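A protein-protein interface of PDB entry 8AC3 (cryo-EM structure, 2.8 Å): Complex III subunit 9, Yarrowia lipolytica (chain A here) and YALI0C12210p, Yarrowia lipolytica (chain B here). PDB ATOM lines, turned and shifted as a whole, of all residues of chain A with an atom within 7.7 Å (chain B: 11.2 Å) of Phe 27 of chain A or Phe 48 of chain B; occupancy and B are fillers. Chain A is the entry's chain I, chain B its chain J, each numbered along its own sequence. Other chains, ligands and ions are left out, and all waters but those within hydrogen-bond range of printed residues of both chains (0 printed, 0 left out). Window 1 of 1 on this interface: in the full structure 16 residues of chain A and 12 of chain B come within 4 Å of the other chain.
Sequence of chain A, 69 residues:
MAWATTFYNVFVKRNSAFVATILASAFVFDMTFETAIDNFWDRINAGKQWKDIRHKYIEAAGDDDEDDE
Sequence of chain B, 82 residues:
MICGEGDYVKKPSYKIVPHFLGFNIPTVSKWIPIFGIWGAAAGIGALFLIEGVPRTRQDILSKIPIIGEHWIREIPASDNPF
The side-chain sulfur (SD) of Met 31 of chain A lies within hydrogen-bond range of a ring nitrogen (NE2) of His 70 of chain B, 3.3 Å away.
The side-chain carboxylate (OE2) of Glu 51 of chain B lies within hydrogen-bond range of the indole nitrogen (NE1) of Trp 71 of chain B, 2.9 Å away. O of His 70 of chain B sits at hydrogen-bond distance from NH1 of Arg 73 of chain B, 3.3 Å away. The side-chain carboxylate (OE2) of Glu 51 of chain B lies within salt-bridge range of the guanidinium group (NH2) of Arg 57 of chain B.
Among the printed residues, pairs that only touch across the chains: Phe 27 of chain A with Phe 48 of chain B (3.5 Å), Leu 23 of chain A with Ala 41 of chain B (3.5 Å), Met 31 of chain A with Glu 51 of chain B (3.7 Å), Ala 26 of chain A with Phe 48 of chain B (3.7 Å), Asp 30 of chain A with Phe 48 of chain B (3.8 Å), Ala 24 of chain A with Ile 44 of chain B (3.8 Å), Leu 23 of chain A with Ile 44 of chain B (3.9 Å) and Met 31 of chain A with Trp 71 of chain B (3.99 Å).
Of the printed residues of chain B, Phe 27 of chain A touches Phe 48 (3.5 Å). Ala 26 of chain A touches one residue of chain B. No residue of chain B comes within 4 Å of Val 28 of chain A. Of chain B, only Phe 48 (3.8 Å) comes within 4 Å of Asp 30 of chain A. Printed residues of chain A within 4 Å of Ala 41 of chain B: Leu 23. Of the printed residues of chain A, Ile 44 of chain B touches Leu 23 (3.9 Å) and Ala 24 (3.8 Å). Of the printed residues of chain A, His 70 of chain B touches Met 31. The nearest residue of chain A that does not touch Phe 48 of chain B is Leu 23 of chain A (4.7 Å). The nearest printed residue of chain B that does not touch Met 31 of chain A is Phe 48 of chain B (4.9 Å).
Of the 13 printed residues of chain A, 6 touch a printed residue of chain B. Hydrophobic or aromatic side chains of chain A that line the printed part of chain B: Leu 23, Ala 26, Phe 27 and Met 31. Printed residues of chain B that touch a printed residue of chain A: Ala 41, Ile 44, Phe 48, Glu 51, His 70 and Trp 71. Among the printed residues, no Asp or Glu carboxylate lies within 4 Å of a Lys or Arg side-chain nitrogen of the other chain.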
ATOM      1  N   THR A  21     -17.406   1.458 -13.284  1.00  0.00           N
ATOM      2  CA  THR A  21     -17.467   0.061 -13.692  1.00  0.00           C
ATOM      3  C   THR A  21     -16.902  -0.103 -15.099  1.00  0.00           C
ATOM      4  O   THR A  21     -16.232  -1.090 -15.371  1.00  0.00           O
ATOM      5  CB  THR A  21     -18.909  -0.450 -13.601  1.00  0.00           C
ATOM      6  OG1 THR A  21     -19.279  -0.318 -12.229  1.00  0.00           O
ATOM      7  CG2 THR A  21     -19.088  -1.883 -14.056  1.00  0.00           C
ATOM      8  N   ILE A  22     -17.204   0.850 -15.987  1.00  0.00           N
ATOM      9  CA  ILE A  22     -16.729   0.811 -17.363  1.00  0.00           C
ATOM     10  C   ILE A  22     -15.205   0.915 -17.351  1.00  0.00           C
ATOM     11  O   ILE A  22     -14.549   0.141 -18.033  1.00  0.00           O
ATOM     12  CB  ILE A  22     -17.419   1.901 -18.217  1.00  0.00           C
ATOM     13  CG1 ILE A  22     -18.851   1.503 -18.597  1.00  0.00           C
ATOM     14  CG2 ILE A  22     -16.602   2.304 -19.442  1.00  0.00           C
ATOM     15  CD1 ILE A  22     -19.758   2.675 -18.939  1.00  0.00           C
ATOM     16  N   LEU A  23     -14.652   1.837 -16.548  1.00  0.00           N
ATOM     17  CA  LEU A  23     -13.213   2.043 -16.529  1.00  0.00           C
ATOM     18  C   LEU A  23     -12.504   0.852 -15.908  1.00  0.00           C
ATOM     19  O   LEU A  23     -11.443   0.479 -16.389  1.00  0.00           O
ATOM     20  CB  LEU A  23     -12.846   3.341 -15.811  1.00  0.00           C
ATOM     21  CG  LEU A  23     -13.366   4.585 -16.521  1.00  0.00           C
ATOM     22  CD1 LEU A  23     -12.996   5.848 -15.767  1.00  0.00           C
ATOM     23  CD2 LEU A  23     -12.896   4.635 -17.968  1.00  0.00           C
ATOM     24  N   ALA A  24     -13.087   0.256 -14.866  1.00  0.00           N
ATOM     25  CA  ALA A  24     -12.459  -0.904 -14.259  1.00  0.00           C
ATOM     26  C   ALA A  24     -12.490  -2.084 -15.231  1.00  0.00           C
ATOM     27  O   ALA A  24     -11.522  -2.837 -15.326  1.00  0.00           O
ATOM     28  CB  ALA A  24     -13.110  -1.218 -12.941  1.00  0.00           C
ATOM     29  N   SER A  25     -13.588  -2.208 -15.981  1.00  0.00           N
ATOM     30  CA  SER A  25     -13.708  -3.236 -17.001  1.00  0.00           C
ATOM     31  C   SER A  25     -12.689  -3.010 -18.112  1.00  0.00           C
ATOM     32  O   SER A  25     -12.135  -3.968 -18.634  1.00  0.00           O
ATOM     33  CB  SER A  25     -15.086  -3.254 -17.559  1.00  0.00           C
ATOM     34  OG  SER A  25     -16.013  -3.553 -16.532  1.00  0.00           O
ATOM     35  N   ALA A  26     -12.478  -1.737 -18.474  1.00  0.00           N
ATOM     36  CA  ALA A  26     -11.539  -1.366 -19.520  1.00  0.00           C
ATOM     37  C   ALA A  26     -10.137  -1.781 -19.103  1.00  0.00           C
ATOM     38  O   ALA A  26      -9.392  -2.292 -19.932  1.00  0.00           O
ATOM     39  CB  ALA A  26     -11.609   0.109 -19.822  1.00  0.00           C
ATOM     40  N   PHE A  27      -9.805  -1.544 -17.830  1.00  0.00           N
ATOM     41  CA  PHE A  27      -8.514  -1.909 -17.280  1.00  0.00           C
ATOM     42  C   PHE A  27      -8.327  -3.418 -17.404  1.00  0.00           C
ATOM     43  O   PHE A  27      -7.294  -3.858 -17.905  1.00  0.00           O
ATOM     44  CB  PHE A  27      -8.410  -1.449 -15.826  1.00  0.00           C
ATOM     45  CG  PHE A  27      -7.025  -1.121 -15.330  1.00  0.00           C
ATOM     46  CD1 PHE A  27      -5.927  -1.921 -15.627  1.00  0.00           C
ATOM     47  CD2 PHE A  27      -6.826  -0.016 -14.515  1.00  0.00           C
ATOM     48  CE1 PHE A  27      -4.663  -1.606 -15.149  1.00  0.00           C
ATOM     49  CE2 PHE A  27      -5.564   0.295 -14.028  1.00  0.00           C
ATOM     50  CZ  PHE A  27      -4.483  -0.498 -14.350  1.00  0.00           C
ATOM     51  N   VAL A  28      -9.343  -4.191 -17.000  1.00  0.00           N
ATOM     52  CA  VAL A  28      -9.214  -5.639 -16.991  1.00  0.00           C
ATOM     53  C   VAL A  28      -9.134  -6.149 -18.424  1.00  0.00           C
ATOM     54  O   VAL A  28      -8.296  -6.992 -18.738  1.00  0.00           O
ATOM     55  CB  VAL A  28     -10.368  -6.304 -16.223  1.00  0.00           C
ATOM     56  CG1 VAL A  28     -10.453  -7.796 -16.488  1.00  0.00           C
ATOM     57  CG2 VAL A  28     -10.287  -6.027 -14.736  1.00  0.00           C
ATOM     58  N   PHE A  29     -10.010  -5.631 -19.284  1.00  0.00           N
ATOM     59  CA  PHE A  29      -9.994  -6.051 -20.669  1.00  0.00           C
ATOM     60  C   PHE A  29      -8.616  -5.783 -21.268  1.00  0.00           C
ATOM     61  O   PHE A  29      -8.002  -6.679 -21.841  1.00  0.00           O
ATOM     62  CB  PHE A  29     -11.066  -5.311 -21.462  1.00  0.00           C
ATOM     63  CG  PHE A  29     -10.968  -5.576 -22.940  1.00  0.00           C
ATOM     64  CD1 PHE A  29     -11.477  -6.750 -23.478  1.00  0.00           C
ATOM     65  CD2 PHE A  29     -10.316  -4.686 -23.784  1.00  0.00           C
ATOM     66  CE1 PHE A  29     -11.371  -7.007 -24.838  1.00  0.00           C
ATOM     67  CE2 PHE A  29     -10.204  -4.948 -25.144  1.00  0.00           C
ATOM     68  CZ  PHE A  29     -10.736  -6.106 -25.670  1.00  0.00           C
ATOM     69  N   ASP A  30      -8.135  -4.548 -21.121  1.00  0.00           N
ATOM     70  CA  ASP A  30      -6.844  -4.157 -21.653  1.00  0.00           C
ATOM     71  C   ASP A  30      -5.747  -5.152 -21.266  1.00  0.00           C
ATOM     72  O   ASP A  30      -4.932  -5.508 -22.114  1.00  0.00           O
ATOM     73  CB  ASP A  30      -6.464  -2.750 -21.200  1.00  0.00           C
ATOM     74  CG  ASP A  30      -5.503  -2.053 -22.152  1.00  0.00           C
ATOM     75  OD1 ASP A  30      -5.951  -1.652 -23.254  1.00  0.00           O
ATOM     76  OD2 ASP A  30      -4.314  -1.906 -21.794  1.00  0.00           O
ATOM     77  N   MET A  31      -5.714  -5.566 -19.994  1.00  0.00           N
ATOM     78  CA  MET A  31      -4.648  -6.412 -19.474  1.00  0.00           C
ATOM     79  C   MET A  31      -4.755  -7.845 -19.992  1.00  0.00           C
ATOM     80  O   MET A  31      -3.756  -8.466 -20.362  1.00  0.00           O
ATOM     81  CB  MET A  31      -4.667  -6.413 -17.944  1.00  0.00           C
ATOM     82  CG  MET A  31      -4.188  -5.109 -17.345  1.00  0.00           C
ATOM     83  SD  MET A  31      -2.642  -4.513 -18.087  1.00  0.00           S
ATOM     84  CE  MET A  31      -3.247  -3.193 -19.137  1.00  0.00           C
ATOM     85  N   THR A  32      -5.978  -8.357 -20.016  1.00  0.00           N
ATOM     86  CA  THR A  32      -6.206  -9.736 -20.385  1.00  0.00           C
ATOM     87  C   THR A  32      -6.110  -9.885 -21.893  1.00  0.00           C
ATOM     88  O   THR A  32      -5.617 -10.897 -22.364  1.00  0.00           O
ATOM     89  CB  THR A  32      -7.548 -10.224 -19.844  1.00  0.00           C
ATOM     90  OG1 THR A  32      -8.523  -9.288 -20.303  1.00  0.00           O
ATOM     91  CG2 THR A  32      -7.545 -10.288 -18.334  1.00  0.00           C
ATOM     92  N   PHE A  33      -6.566  -8.878 -22.636  1.00  0.00           N
ATOM     93  CA  PHE A  33      -6.591  -8.987 -24.083  1.00  0.00           C
ATOM     94  C   PHE A  33      -5.165  -8.972 -24.617  1.00  0.00           C
ATOM     95  O   PHE A  33      -4.857  -9.666 -25.581  1.00  0.00           O
ATOM     96  CB  PHE A  33      -7.411  -7.839 -24.661  1.00  0.00           C
ATOM     97  CG  PHE A  33      -7.549  -7.804 -26.158  1.00  0.00           C
ATOM     98  CD1 PHE A  33      -8.163  -8.845 -26.845  1.00  0.00           C
ATOM     99  CD2 PHE A  33      -7.140  -6.685 -26.875  1.00  0.00           C
ATOM    100  CE1 PHE A  33      -8.334  -8.780 -28.222  1.00  0.00           C
ATOM    101  CE2 PHE A  33      -7.298  -6.627 -28.253  1.00  0.00           C
ATOM    102  CZ  PHE A  33      -7.901  -7.671 -28.924  1.00  0.00           C
ATOM    103  N   GLY B  39     -14.456   9.777  -7.303  1.00  0.00           N
ATOM    104  CA  GLY B  39     -13.048   9.816  -6.941  1.00  0.00           C
ATOM    105  C   GLY B  39     -12.371   8.497  -7.294  1.00  0.00           C
ATOM    106  O   GLY B  39     -11.251   8.487  -7.804  1.00  0.00           O
ATOM    107  N   ALA B  40     -13.088   7.397  -7.022  1.00  0.00           N
ATOM    108  CA  ALA B  40     -12.688   6.056  -7.419  1.00  0.00           C
ATOM    109  C   ALA B  40     -12.567   5.977  -8.938  1.00  0.00           C
ATOM    110  O   ALA B  40     -11.576   5.457  -9.440  1.00  0.00           O
ATOM    111  CB  ALA B  40     -13.653   5.020  -6.889  1.00  0.00           C
ATOM    112  N   ALA B  41     -13.578   6.490  -9.651  1.00  0.00           N
ATOM    113  CA  ALA B  41     -13.583   6.469 -11.103  1.00  0.00           C
ATOM    114  C   ALA B  41     -12.366   7.226 -11.623  1.00  0.00           C
ATOM    115  O   ALA B  41     -11.744   6.790 -12.584  1.00  0.00           O
ATOM    116  CB  ALA B  41     -14.868   7.052 -11.641  1.00  0.00           C
ATOM    117  N   ALA B  42     -12.048   8.355 -10.979  1.00  0.00           N
ATOM    118  CA  ALA B  42     -10.929   9.178 -11.407  1.00  0.00           C
ATOM    119  C   ALA B  42      -9.616   8.476 -11.068  1.00  0.00           C
ATOM    120  O   ALA B  42      -8.669   8.538 -11.849  1.00  0.00           O
ATOM    121  CB  ALA B  42     -11.013  10.561 -10.810  1.00  0.00           C
ATOM    122  N   GLY B  43      -9.584   7.788  -9.920  1.00  0.00           N
ATOM    123  CA  GLY B  43      -8.414   7.038  -9.496  1.00  0.00           C
ATOM    124  C   GLY B  43      -8.112   5.883 -10.450  1.00  0.00           C
ATOM    125  O   GLY B  43      -6.996   5.787 -10.953  1.00  0.00           O
ATOM    126  N   ILE B  44      -9.119   5.027 -10.682  1.00  0.00           N
ATOM    127  CA  ILE B  44      -9.038   3.908 -11.613  1.00  0.00           C
ATOM    128  C   ILE B  44      -8.596   4.438 -12.973  1.00  0.00           C
ATOM    129  O   ILE B  44      -7.675   3.892 -13.567  1.00  0.00           O
ATOM    130  CB  ILE B  44     -10.378   3.140 -11.690  1.00  0.00           C
ATOM    131  CG1 ILE B  44     -10.666   2.379 -10.392  1.00  0.00           C
ATOM    132  CG2 ILE B  44     -10.434   2.216 -12.902  1.00  0.00           C
ATOM    133  CD1 ILE B  44     -12.138   2.105 -10.137  1.00  0.00           C
ATOM    134  N   GLY B  45      -9.243   5.516 -13.437  1.00  0.00           N
ATOM    135  CA  GLY B  45      -8.990   6.055 -14.764  1.00  0.00           C
ATOM    136  C   GLY B  45      -7.575   6.610 -14.894  1.00  0.00           C
ATOM    137  O   GLY B  45      -6.909   6.382 -15.905  1.00  0.00           O
ATOM    138  N   ALA B  46      -7.127   7.333 -13.861  1.00  0.00           N
ATOM    139  CA  ALA B  46      -5.815   7.954 -13.904  1.00  0.00           C
ATOM    140  C   ALA B  46      -4.758   6.861 -13.928  1.00  0.00           C
ATOM    141  O   ALA B  46      -3.849   6.901 -14.752  1.00  0.00           O
ATOM    142  CB  ALA B  46      -5.619   8.891 -12.738  1.00  0.00           C
ATOM    143  N   LEU B  47      -4.932   5.873 -13.048  1.00  0.00           N
ATOM    144  CA  LEU B  47      -3.965   4.804 -12.888  1.00  0.00           C
ATOM    145  C   LEU B  47      -3.886   3.996 -14.177  1.00  0.00           C
ATOM    146  O   LEU B  47      -2.802   3.588 -14.580  1.00  0.00           O
ATOM    147  CB  LEU B  47      -4.384   3.932 -11.704  1.00  0.00           C
ATOM    148  CG  LEU B  47      -3.545   2.682 -11.462  1.00  0.00           C
ATOM    149  CD1 LEU B  47      -2.182   3.048 -10.890  1.00  0.00           C
ATOM    150  CD2 LEU B  47      -4.278   1.736 -10.524  1.00  0.00           C
ATOM    151  N   PHE B  48      -5.046   3.789 -14.805  1.00  0.00           N
ATOM    152  CA  PHE B  48      -5.169   3.131 -16.094  1.00  0.00           C
ATOM    153  C   PHE B  48      -4.389   3.884 -17.169  1.00  0.00           C
ATOM    154  O   PHE B  48      -3.742   3.247 -17.992  1.00  0.00           O
ATOM    155  CB  PHE B  48      -6.647   3.016 -16.457  1.00  0.00           C
ATOM    156  CG  PHE B  48      -6.948   2.295 -17.743  1.00  0.00           C
ATOM    157  CD1 PHE B  48      -6.263   1.139 -18.108  1.00  0.00           C
ATOM    158  CD2 PHE B  48      -7.957   2.754 -18.578  1.00  0.00           C
ATOM    159  CE1 PHE B  48      -6.561   0.478 -19.293  1.00  0.00           C
ATOM    160  CE2 PHE B  48      -8.265   2.084 -19.756  1.00  0.00           C
ATOM    161  CZ  PHE B  48      -7.566   0.950 -20.113  1.00  0.00           C
ATOM    162  N   LEU B  49      -4.457   5.225 -17.164  1.00  0.00           N
ATOM    163  CA  LEU B  49      -3.779   6.044 -18.163  1.00  0.00           C
ATOM    164  C   LEU B  49      -2.264   5.943 -18.028  1.00  0.00           C
ATOM    165  O   LEU B  49      -1.543   6.113 -19.009  1.00  0.00           O
ATOM    166  CB  LEU B  49      -4.188   7.508 -18.017  1.00  0.00           C
ATOM    167  CG  LEU B  49      -5.424   7.942 -18.796  1.00  0.00           C
ATOM    168  CD1 LEU B  49      -5.758   9.383 -18.450  1.00  0.00           C
ATOM    169  CD2 LEU B  49      -5.212   7.804 -20.298  1.00  0.00           C
ATOM    170  N   ILE B  50      -1.774   5.721 -16.806  1.00  0.00           N
ATOM    171  CA  ILE B  50      -0.332   5.729 -16.623  1.00  0.00           C
ATOM    172  C   ILE B  50       0.173   4.321 -16.337  1.00  0.00           C
ATOM    173  O   ILE B  50       1.274   4.144 -15.821  1.00  0.00           O
ATOM    174  CB  ILE B  50       0.107   6.721 -15.538  1.00  0.00           C
ATOM    175  CG1 ILE B  50      -0.516   6.374 -14.183  1.00  0.00           C
ATOM    176  CG2 ILE B  50      -0.152   8.155 -15.986  1.00  0.00           C
ATOM    177  CD1 ILE B  50       0.185   7.002 -13.001  1.00  0.00           C
ATOM    178  N   GLU B  51      -0.623   3.326 -16.712  1.00  0.00           N
ATOM    179  CA  GLU B  51      -0.263   1.945 -16.459  1.00  0.00           C
ATOM    180  C   GLU B  51       1.023   1.632 -17.217  1.00  0.00           C
ATOM    181  O   GLU B  51       1.802   0.786 -16.794  1.00  0.00           O
ATOM    182  CB  GLU B  51      -1.440   1.059 -16.861  1.00  0.00           C
ATOM    183  CG  GLU B  51      -1.149  -0.436 -16.893  1.00  0.00           C
ATOM    184  CD  GLU B  51      -0.415  -1.041 -18.088  1.00  0.00           C
ATOM    185  OE1 GLU B  51      -0.595  -0.553 -19.231  1.00  0.00           O
ATOM    186  OE2 GLU B  51       0.332  -2.028 -17.878  1.00  0.00           O
ATOM    187  N   GLY B  52       1.212   2.304 -18.354  1.00  0.00           N
ATOM    188  CA  GLY B  52       2.366   2.073 -19.203  1.00  0.00           C
ATOM    189  C   GLY B  52       3.652   2.664 -18.626  1.00  0.00           C
ATOM    190  O   GLY B  52       4.727   2.116 -18.848  1.00  0.00           O
ATOM    191  N   VAL B  53       3.545   3.769 -17.887  1.00  0.00           N
ATOM    192  CA  VAL B  53       4.710   4.389 -17.274  1.00  0.00           C
ATOM    193  C   VAL B  53       5.451   3.379 -16.398  1.00  0.00           C
ATOM    194  O   VAL B  53       4.846   2.777 -15.518  1.00  0.00           O
ATOM    195  CB  VAL B  53       4.296   5.618 -16.458  1.00  0.00           C
ATOM    196  CG1 VAL B  53       5.496   6.242 -15.760  1.00  0.00           C
ATOM    197  CG2 VAL B  53       3.560   6.612 -17.334  1.00  0.00           C
ATOM    198  N   PRO B  54       6.764   3.125 -16.631  1.00  0.00           N
ATOM    199  CA  PRO B  54       7.505   2.101 -15.889  1.00  0.00           C
ATOM    200  C   PRO B  54       7.549   2.289 -14.377  1.00  0.00           C
ATOM    201  O   PRO B  54       7.550   1.306 -13.636  1.00  0.00           O
ATOM    202  CB  PRO B  54       8.919   2.168 -16.476  1.00  0.00           C
ATOM    203  CG  PRO B  54       8.678   2.685 -17.868  1.00  0.00           C
ATOM    204  CD  PRO B  54       7.573   3.709 -17.711  1.00  0.00           C
ATOM    205  N   THR B  56       5.067   3.613 -12.604  1.00  0.00           N
ATOM    206  CA  THR B  56       3.766   3.176 -12.121  1.00  0.00           C
ATOM    207  C   THR B  56       3.791   1.677 -11.860  1.00  0.00           C
ATOM    208  O   THR B  56       3.153   1.205 -10.932  1.00  0.00           O
ATOM    209  CB  THR B  56       2.667   3.413 -13.164  1.00  0.00           C
ATOM    210  OG1 THR B  56       2.779   4.785 -13.528  1.00  0.00           O
ATOM    211  CG2 THR B  56       1.260   3.093 -12.694  1.00  0.00           C
ATOM    212  N   ARG B  57       4.484   0.930 -12.718  1.00  0.00           N
ATOM    213  CA  ARG B  57       4.485  -0.516 -12.595  1.00  0.00           C
ATOM    214  C   ARG B  57       5.352  -0.888 -11.406  1.00  0.00           C
ATOM    215  O   ARG B  57       4.921  -1.626 -10.523  1.00  0.00           O
ATOM    216  CB  ARG B  57       5.018  -1.163 -13.867  1.00  0.00           C
ATOM    217  CG  ARG B  57       4.316  -0.640 -15.102  1.00  0.00           C
ATOM    218  CD  ARG B  57       4.771  -1.325 -16.336  1.00  0.00           C
ATOM    219  NE  ARG B  57       3.780  -1.160 -17.379  1.00  0.00           N
ATOM    220  CZ  ARG B  57       3.957  -1.667 -18.580  1.00  0.00           C
ATOM    221  NH1 ARG B  57       5.079  -2.317 -18.844  1.00  0.00           N
ATOM    222  NH2 ARG B  57       3.040  -1.516 -19.518  1.00  0.00           N
ATOM    223  N   ILE B  60       3.603   0.901  -8.032  1.00  0.00           N
ATOM    224  CA  ILE B  60       2.220   0.641  -7.648  1.00  0.00           C
ATOM    225  C   ILE B  60       1.825  -0.770  -8.072  1.00  0.00           C
ATOM    226  O   ILE B  60       1.501  -1.613  -7.238  1.00  0.00           O
ATOM    227  CB  ILE B  60       1.216   1.653  -8.247  1.00  0.00           C
ATOM    228  CG1 ILE B  60       1.584   3.140  -8.132  1.00  0.00           C
ATOM    229  CG2 ILE B  60      -0.193   1.348  -7.756  1.00  0.00           C
ATOM    230  CD1 ILE B  60       1.922   3.627  -6.736  1.00  0.00           C
ATOM    231  N   LEU B  61       1.806  -0.999  -9.386  1.00  0.00           N
ATOM    232  CA  LEU B  61       1.077  -2.119  -9.952  1.00  0.00           C
ATOM    233  C   LEU B  61       1.707  -3.464  -9.603  1.00  0.00           C
ATOM    234  O   LEU B  61       0.986  -4.439  -9.426  1.00  0.00           O
ATOM    235  CB  LEU B  61       0.949  -1.929 -11.464  1.00  0.00           C
ATOM    236  CG  LEU B  61       0.009  -0.798 -11.874  1.00  0.00           C
ATOM    237  CD1 LEU B  61      -0.016  -0.623 -13.383  1.00  0.00           C
ATOM    238  CD2 LEU B  61      -1.395  -1.033 -11.336  1.00  0.00           C
ATOM    239  N   SER B  62       3.037  -3.520  -9.502  1.00  0.00           N
ATOM    240  CA  SER B  62       3.710  -4.788  -9.269  1.00  0.00           C
ATOM    241  C   SER B  62       3.605  -5.222  -7.804  1.00  0.00           C
ATOM    242  O   SER B  62       3.927  -6.365  -7.475  1.00  0.00           O
ATOM    243  CB  SER B  62       5.131  -4.733  -9.752  1.00  0.00           C
ATOM    244  OG  SER B  62       5.907  -3.857  -8.946  1.00  0.00           O
ATOM    245  N   ILE B  64       0.690  -5.040  -6.019  1.00  0.00           N
ATOM    246  CA  ILE B  64      -0.629  -5.626  -5.804  1.00  0.00           C
ATOM    247  C   ILE B  64      -0.475  -7.143  -5.674  1.00  0.00           C
ATOM    248  O   ILE B  64       0.184  -7.767  -6.506  1.00  0.00           O
ATOM    249  CB  ILE B  64      -1.612  -5.221  -6.931  1.00  0.00           C
ATOM    250  CG1 ILE B  64      -1.769  -3.701  -7.038  1.00  0.00           C
ATOM    251  CG2 ILE B  64      -2.964  -5.918  -6.809  1.00  0.00           C
ATOM    252  CD1 ILE B  64      -2.318  -3.224  -8.367  1.00  0.00           C
ATOM    253  N   ILE B  67      -2.010 -10.517  -8.567  1.00  0.00           N
ATOM    254  CA  ILE B  67      -2.155  -9.824  -9.841  1.00  0.00           C
ATOM    255  C   ILE B  67      -0.822  -9.174 -10.244  1.00  0.00           C
ATOM    256  O   ILE B  67      -0.490  -9.084 -11.432  1.00  0.00           O
ATOM    257  CB  ILE B  67      -3.335  -8.826  -9.694  1.00  0.00           C
ATOM    258  CG1 ILE B  67      -4.616  -9.537  -9.236  1.00  0.00           C
ATOM    259  CG2 ILE B  67      -3.594  -8.015 -10.959  1.00  0.00           C
ATOM    260  CD1 ILE B  67      -5.619  -8.656  -8.502  1.00  0.00           C
ATOM    261  N   GLY B  68      -0.024  -8.786  -9.238  1.00  0.00           N
ATOM    262  CA  GLY B  68       1.126  -7.907  -9.398  1.00  0.00           C
ATOM    263  C   GLY B  68       2.247  -8.461 -10.273  1.00  0.00           C
ATOM    264  O   GLY B  68       3.104  -7.707 -10.715  1.00  0.00           O
ATOM    265  N   HIS B  70       1.923  -9.646 -13.130  1.00  0.00           N
ATOM    266  CA  HIS B  70       1.618  -9.270 -14.502  1.00  0.00           C
ATOM    267  C   HIS B  70       2.575  -8.176 -14.977  1.00  0.00           C
ATOM    268  O   HIS B  70       2.861  -8.088 -16.169  1.00  0.00           O
ATOM    269  CB  HIS B  70       0.140  -8.879 -14.653  1.00  0.00           C
ATOM    270  CG  HIS B  70      -0.199  -8.343 -16.004  1.00  0.00           C
ATOM    271  ND1 HIS B  70      -0.411  -9.161 -17.097  1.00  0.00           N
ATOM    272  CD2 HIS B  70      -0.340  -7.075 -16.448  1.00  0.00           C
ATOM    273  CE1 HIS B  70      -0.672  -8.416 -18.155  1.00  0.00           C
ATOM    274  NE2 HIS B  70      -0.632  -7.132 -17.784  1.00  0.00           N
ATOM    275  N   TRP B  71       3.083  -7.370 -14.035  1.00  0.00           N
ATOM    276  CA  TRP B  71       3.863  -6.191 -14.379  1.00  0.00           C
ATOM    277  C   TRP B  71       5.348  -6.352 -14.064  1.00  0.00           C
ATOM    278  O   TRP B  71       6.119  -5.406 -14.234  1.00  0.00           O
ATOM    279  CB  TRP B  71       3.292  -4.958 -13.689  1.00  0.00           C
ATOM    280  CG  TRP B  71       1.964  -4.550 -14.235  1.00  0.00           C
ATOM    281  CD1 TRP B  71       1.722  -3.859 -15.386  1.00  0.00           C
ATOM    282  CD2 TRP B  71       0.686  -4.810 -13.643  1.00  0.00           C
ATOM    283  NE1 TRP B  71       0.377  -3.675 -15.552  1.00  0.00           N
ATOM    284  CE2 TRP B  71      -0.285  -4.244 -14.501  1.00  0.00           C
ATOM    285  CE3 TRP B  71       0.272  -5.469 -12.480  1.00  0.00           C
ATOM    286  CZ2 TRP B  71      -1.648  -4.301 -14.224  1.00  0.00           C
ATOM    287  CZ3 TRP B  71      -1.075  -5.512 -12.199  1.00  0.00           C
ATOM    288  CH2 TRP B  71      -2.017  -4.947 -13.066  1.00  0.00           C
ATOM    289  N   ARG B  73       8.186  -7.927 -15.585  1.00  0.00           N
ATOM    290  CA  ARG B  73       8.632  -8.559 -16.816  1.00  0.00           C
ATOM    291  C   ARG B  73      10.040  -8.076 -17.152  1.00  0.00           C
ATOM    292  O   ARG B  73      10.295  -6.871 -17.194  1.00  0.00           O
ATOM    293  CB  ARG B  73       7.637  -8.314 -17.955  1.00  0.00           C
ATOM    294  CG  ARG B  73       6.952  -6.956 -17.906  1.00  0.00           C
ATOM    295  CD  ARG B  73       6.262  -6.608 -19.204  1.00  0.00           C
ATOM    296  NE  ARG B  73       5.112  -5.750 -18.948  1.00  0.00           N
ATOM    297  CZ  ARG B  73       3.838  -6.135 -19.003  1.00  0.00           C
ATOM    298  NH1 ARG B  73       3.531  -7.381 -19.324  1.00  0.00           N
ATOM    299  NH2 ARG B  73       2.874  -5.268 -18.747  1.00  0.00           N
